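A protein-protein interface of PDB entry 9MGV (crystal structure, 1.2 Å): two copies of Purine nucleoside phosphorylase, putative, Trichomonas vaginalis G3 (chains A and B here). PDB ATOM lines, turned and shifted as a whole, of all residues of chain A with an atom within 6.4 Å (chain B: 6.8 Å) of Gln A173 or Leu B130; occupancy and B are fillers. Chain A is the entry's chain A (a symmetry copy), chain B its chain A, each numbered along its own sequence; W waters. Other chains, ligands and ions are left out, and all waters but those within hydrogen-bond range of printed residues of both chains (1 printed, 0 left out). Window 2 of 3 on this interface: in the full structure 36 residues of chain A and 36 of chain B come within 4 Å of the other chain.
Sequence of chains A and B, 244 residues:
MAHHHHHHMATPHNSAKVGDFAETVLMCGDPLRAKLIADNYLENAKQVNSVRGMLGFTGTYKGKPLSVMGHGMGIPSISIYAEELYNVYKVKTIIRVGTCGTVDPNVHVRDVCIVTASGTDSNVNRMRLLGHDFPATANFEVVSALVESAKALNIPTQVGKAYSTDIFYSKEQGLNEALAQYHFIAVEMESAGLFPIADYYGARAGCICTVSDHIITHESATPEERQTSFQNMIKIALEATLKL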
ATOM      1  N   SER A 170      17.671 -17.624   2.454  1.00  0.00           N
ATOM      2  CA  SER A 170      18.099 -18.969   2.788  1.00  0.00           C
ATOM      3  C   SER A 170      16.989 -19.778   3.433  1.00  0.00           C
ATOM      4  O   SER A 170      16.263 -19.291   4.298  1.00  0.00           O
ATOM      5  CB  SER A 170      19.272 -18.923   3.759  1.00  0.00           C
ATOM      6  OG  SER A 170      19.670 -20.246   4.079  1.00  0.00           O
ATOM      7  N   LYS A 171      16.927 -21.044   3.038  1.00  0.00           N
ATOM      8  CA  LYS A 171      16.057 -22.055   3.616  1.00  0.00           C
ATOM      9  C   LYS A 171      16.893 -23.209   4.171  1.00  0.00           C
ATOM     10  O   LYS A 171      16.361 -24.282   4.476  1.00  0.00           O
ATOM     11  CB  LYS A 171      15.061 -22.542   2.555  1.00  0.00           C
ATOM     12  CG  LYS A 171      14.173 -21.422   2.016  1.00  0.00           C
ATOM     13  CD  LYS A 171      13.381 -21.811   0.775  1.00  0.00           C
ATOM     14  CE  LYS A 171      12.449 -20.716   0.288  1.00  0.00           C
ATOM     15  NZ  LYS A 171      13.175 -19.465  -0.065  1.00  0.00           N
ATOM     16  N   GLU A 172      18.199 -22.997   4.340  1.00  0.00           N
ATOM     17  CA  GLU A 172      19.164 -24.080   4.534  1.00  0.00           C
ATOM     18  C   GLU A 172      19.391 -24.357   6.014  1.00  0.00           C
ATOM     19  O   GLU A 172      20.025 -23.573   6.717  1.00  0.00           O
ATOM     20  CB  GLU A 172      20.475 -23.708   3.844  1.00  0.00           C
ATOM     21  CG  GLU A 172      21.487 -24.816   3.816  1.00  0.00           C
ATOM     22  CD  GLU A 172      22.752 -24.460   3.074  1.00  0.00           C
ATOM     23  OE1 GLU A 172      22.906 -23.287   2.629  1.00  0.00           O
ATOM     24  OE2 GLU A 172      23.614 -25.357   2.988  1.00  0.00           O
ATOM     25  N   GLN A 173      18.936 -25.513   6.461  1.00  0.00           N
ATOM     26  CA  GLN A 173      19.066 -25.892   7.860  1.00  0.00           C
ATOM     27  C   GLN A 173      20.516 -26.181   8.217  1.00  0.00           C
ATOM     28  O   GLN A 173      21.237 -26.852   7.475  1.00  0.00           O
ATOM     29  CB  GLN A 173      18.224 -27.137   8.121  1.00  0.00           C
ATOM     30  CG  GLN A 173      16.774 -26.960   7.749  1.00  0.00           C
ATOM     31  CD  GLN A 173      16.211 -25.650   8.267  1.00  0.00           C
ATOM     32  OE1 GLN A 173      15.856 -24.754   7.484  1.00  0.00           O
ATOM     33  NE2 GLN A 173      16.164 -25.509   9.581  1.00  0.00           N
ATOM     34  N   GLY A 174      20.950 -25.659   9.365  1.00  0.00           N
ATOM     35  CA  GLY A 174      22.282 -25.914   9.858  1.00  0.00           C
ATOM     36  C   GLY A 174      23.355 -24.963   9.367  1.00  0.00           C
ATOM     37  O   GLY A 174      24.480 -25.009   9.882  1.00  0.00           O
ATOM     38  N   LEU A 175      23.049 -24.099   8.393  1.00  0.00           N
ATOM     39  CA  LEU A 175      24.056 -23.196   7.843  1.00  0.00           C
ATOM     40  C   LEU A 175      24.533 -22.198   8.891  1.00  0.00           C
ATOM     41  O   LEU A 175      25.743 -22.002   9.079  1.00  0.00           O
ATOM     42  CB  LEU A 175      23.486 -22.465   6.628  1.00  0.00           C
ATOM     43  CG  LEU A 175      24.443 -21.447   5.991  1.00  0.00           C
ATOM     44  CD1 LEU A 175      25.667 -22.144   5.408  1.00  0.00           C
ATOM     45  CD2 LEU A 175      23.729 -20.624   4.946  1.00  0.00           C
ATOM     46  N   ASN A 176      23.594 -21.532   9.571  1.00  0.00           N
ATOM     47  CA  ASN A 176      24.008 -20.507  10.520  1.00  0.00           C
ATOM     48  C   ASN A 176      24.830 -21.105  11.648  1.00  0.00           C
ATOM     49  O   ASN A 176      25.792 -20.486  12.118  1.00  0.00           O
ATOM     50  CB  ASN A 176      22.803 -19.776  11.086  1.00  0.00           C
ATOM     51  CG  ASN A 176      22.117 -18.917  10.058  1.00  0.00           C
ATOM     52  OD1 ASN A 176      22.738 -18.451   9.100  1.00  0.00           O
ATOM     53  ND2 ASN A 176      20.827 -18.690  10.257  1.00  0.00           N
ATOM     54  N   GLU A 177      24.481 -22.318  12.080  1.00  0.00           N
ATOM     55  CA  GLU A 177      25.233 -22.966  13.143  1.00  0.00           C
ATOM     56  C   GLU A 177      26.668 -23.256  12.710  1.00  0.00           C
ATOM     57  O   GLU A 177      27.609 -23.094  13.498  1.00  0.00           O
ATOM     58  CB  GLU A 177      24.526 -24.258  13.540  1.00  0.00           C
ATOM     59  CG  GLU A 177      23.219 -24.065  14.291  1.00  0.00           C
ATOM     60  CD  GLU A 177      21.991 -23.748  13.415  1.00  0.00           C
ATOM     61  OE1 GLU A 177      22.039 -23.658  12.165  1.00  0.00           O
ATOM     62  OE2 GLU A 177      20.909 -23.617  14.013  1.00  0.00           O
ATOM     63  N   ALA A 178      26.863 -23.701  11.470  1.00  0.00           N
ATOM     64  CA  ALA A 178      28.205 -23.979  10.973  1.00  0.00           C
ATOM     65  C   ALA A 178      28.997 -22.693  10.793  1.00  0.00           C
ATOM     66  O   ALA A 178      30.184 -22.636  11.135  1.00  0.00           O
ATOM     67  CB  ALA A 178      28.113 -24.770   9.666  1.00  0.00           C
ATOM     68  N   ASN B 125      37.160 -29.878   4.521  1.00  0.00           N
ATOM     69  CA  ASN B 125      36.528 -28.587   4.813  1.00  0.00           C
ATOM     70  C   ASN B 125      35.112 -28.513   4.266  1.00  0.00           C
ATOM     71  O   ASN B 125      34.236 -27.899   4.897  1.00  0.00           O
ATOM     72  CB  ASN B 125      37.442 -27.461   4.360  1.00  0.00           C
ATOM     73  CG  ASN B 125      38.746 -27.480   5.132  1.00  0.00           C
ATOM     74  OD1 ASN B 125      38.782 -27.925   6.276  1.00  0.00           O
ATOM     75  ND2 ASN B 125      39.814 -27.025   4.516  1.00  0.00           N
ATOM     76  N   ARG B 126      34.850 -29.152   3.125  1.00  0.00           N
ATOM     77  CA  ARG B 126      33.474 -29.264   2.657  1.00  0.00           C
ATOM     78  C   ARG B 126      32.615 -29.920   3.721  1.00  0.00           C
ATOM     79  O   ARG B 126      31.481 -29.507   3.970  1.00  0.00           O
ATOM     80  CB  ARG B 126      33.425 -30.045   1.345  1.00  0.00           C
ATOM     81  CG  ARG B 126      34.084 -29.305   0.212  1.00  0.00           C
ATOM     82  CD  ARG B 126      34.090 -30.047  -1.087  1.00  0.00           C
ATOM     83  NE  ARG B 126      34.898 -29.304  -2.032  1.00  0.00           N
ATOM     84  CZ  ARG B 126      34.998 -29.539  -3.323  1.00  0.00           C
ATOM     85  NH1 ARG B 126      34.371 -30.553  -3.884  1.00  0.00           N
ATOM     86  NH2 ARG B 126      35.751 -28.736  -4.065  1.00  0.00           N
ATOM     87  N   MET B 127      33.150 -30.948   4.373  1.00  0.00           N
ATOM     88  CA  MET B 127      32.393 -31.650   5.392  1.00  0.00           C
ATOM     89  C   MET B 127      32.026 -30.763   6.572  1.00  0.00           C
ATOM     90  O   MET B 127      31.034 -31.032   7.257  1.00  0.00           O
ATOM     91  CB  MET B 127      33.180 -32.828   5.936  1.00  0.00           C
ATOM     92  CG  MET B 127      32.469 -33.392   7.137  1.00  0.00           C
ATOM     93  SD  MET B 127      33.171 -34.931   7.684  1.00  0.00           S
ATOM     94  CE  MET B 127      32.793 -35.985   6.275  1.00  0.00           C
ATOM     95  N   ARG B 128      32.808 -29.717   6.834  1.00  0.00           N
ATOM     96  CA  ARG B 128      32.559 -28.817   7.952  1.00  0.00           C
ATOM     97  C   ARG B 128      31.525 -27.744   7.629  1.00  0.00           C
ATOM     98  O   ARG B 128      30.975 -27.139   8.551  1.00  0.00           O
ATOM     99  CB  ARG B 128      33.869 -28.145   8.363  1.00  0.00           C
ATOM    100  CG  ARG B 128      34.889 -29.103   8.951  1.00  0.00           C
ATOM    101  CD  ARG B 128      36.246 -28.419   9.187  1.00  0.00           C
ATOM    102  NE  ARG B 128      37.097 -29.233  10.043  1.00  0.00           N
ATOM    103  CZ  ARG B 128      38.233 -29.825   9.721  1.00  0.00           C
ATOM    104  NH1 ARG B 128      38.819 -29.632   8.547  1.00  0.00           N
ATOM    105  NH2 ARG B 128      38.802 -30.634  10.611  1.00  0.00           N
ATOM    106  N   LEU B 129      31.269 -27.471   6.356  1.00  0.00           N
ATOM    107  CA  LEU B 129      30.432 -26.342   5.958  1.00  0.00           C
ATOM    108  C   LEU B 129      29.382 -26.770   4.938  1.00  0.00           C
ATOM    109  O   LEU B 129      29.167 -26.127   3.908  1.00  0.00           O
ATOM    110  CB  LEU B 129      31.290 -25.178   5.465  1.00  0.00           C
ATOM    111  CG  LEU B 129      30.579 -23.823   5.425  1.00  0.00           C
ATOM    112  CD1 LEU B 129      29.996 -23.397   6.737  1.00  0.00           C
ATOM    113  CD2 LEU B 129      31.511 -22.750   4.876  1.00  0.00           C
ATOM    114  N   LEU B 130      28.685 -27.866   5.242  1.00  0.00           N
ATOM    115  CA  LEU B 130      27.501 -28.285   4.487  1.00  0.00           C
ATOM    116  C   LEU B 130      27.806 -28.495   3.012  1.00  0.00           C
ATOM    117  O   LEU B 130      26.943 -28.292   2.151  1.00  0.00           O
ATOM    118  CB  LEU B 130      26.329 -27.323   4.691  1.00  0.00           C
ATOM    119  CG  LEU B 130      25.785 -27.305   6.109  1.00  0.00           C
ATOM    120  CD1 LEU B 130      24.728 -26.198   6.209  1.00  0.00           C
ATOM    121  CD2 LEU B 130      25.178 -28.614   6.522  1.00  0.00           C
ATOM    122  N   GLY B 131      29.033 -28.922   2.711  1.00  0.00           N
ATOM    123  CA  GLY B 131      29.430 -29.200   1.351  1.00  0.00           C
ATOM    124  C   GLY B 131      29.914 -28.004   0.568  1.00  0.00           C
ATOM    125  O   GLY B 131      30.256 -28.165  -0.606  1.00  0.00           O
ATOM    126  N   HIS B 132      29.956 -26.821   1.170  1.00  0.00           N
ATOM    127  CA  HIS B 132      30.265 -25.585   0.462  1.00  0.00           C
ATOM    128  C   HIS B 132      31.772 -25.305   0.512  1.00  0.00           C
ATOM    129  O   HIS B 132      32.561 -26.140   0.975  1.00  0.00           O
ATOM    130  CB  HIS B 132      29.434 -24.452   1.051  1.00  0.00           C
ATOM    131  CG  HIS B 132      27.970 -24.735   1.065  1.00  0.00           C
ATOM    132  ND1 HIS B 132      27.271 -25.129  -0.055  1.00  0.00           N
ATOM    133  CD2 HIS B 132      27.068 -24.679   2.075  1.00  0.00           C
ATOM    134  CE1 HIS B 132      25.996 -25.287   0.263  1.00  0.00           C
ATOM    135  NE2 HIS B 132      25.847 -25.030   1.553  1.00  0.00           N
HETATM  136  O   HOH W   1      24.990 -21.667   1.771  1.00  0.00           O
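No position is printed for both chains. Of the 7 pairs that touch across the chains among the printed residues, none has its exchanged pair printed and touching as well.
Among the printed residues, pairs that only touch across the chains: Glu A172 with Leu B130 (3.5 Å), Gln A173 with Leu B130 (3.8 Å), Gly A174 with Leu B130 (3.7 Å), Leu A175 with Leu B130 (3.5 Å), Ala A178 with Arg B128 (3.9 Å) and Ala A178 with Leu B129 (3.7 Å).
Water W1 lies within hydrogen-bond range of OE1 of Glu A172 and NE2 of His B132.
The guanidinium group (NH1) of Arg B128 is in hydrogen-bond range of the side-chain amide oxygen (OD1) of Asn B125 (2.8 Å). The backbone carbonyl oxygen (O) of Leu B130 sits at hydrogen-bond distance from a ring nitrogen (NE2) of His B132 (3.5 Å). The side-chain hydroxyl of Ser A170 is in hydrogen-bond range of the backbone NH of Glu A172 (3.1 Å). The side-chain amide oxygen (OE1) of Gln A173 lies close to the backbone carbonyl oxygen (O) of Lys A171, 3.1 Å away.
A ring nitrogen (NE2) of His B132 lies within hydrogen-bond range of the side-chain carboxylate (OE2) of Glu A172 (2.7 Å).
Of the printed residues of chain B, Gln A173 touches Leu B130. Of the printed residues of chain B, Ala A178 touches Arg B128 (3.9 Å) and Leu B129 (3.7 Å). Printed residues of chain B within 4 Å of Glu A172: Leu B130 and His B132. The nearest printed residue of chain B that does not touch Gln A173 is His B132 (7.7 Å). The nearest printed residue of chain A that does not touch Leu B130 is Ala A178 (4.9 Å). The nearest printed residue of chain B that does not touch Glu A172 is Leu B129 (5.7 Å).
Of the 8 printed residues of chain B, 4 touch a printed residue of chain A. Printed residues of chain B that touch a printed residue of chain A: Arg B128, Leu B129, Leu B130 and His B132. Printed residues of chain A that touch a printed residue of chain B: Glu A172, Gln A173, Gly A174, Leu A175 and Ala A178. Hydrophobic or aromatic side chains of chain A within 4 Å of the printed part of chain B: Leu A175 and Ala A178. Along chain A the printed residues that touch a printed residue of chain B span positions 172 to 178. Among the printed residues, no Asp or Glu carboxylate lies within 4 Å of a Lys or Arg side-chain nitrogen of the other chain.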
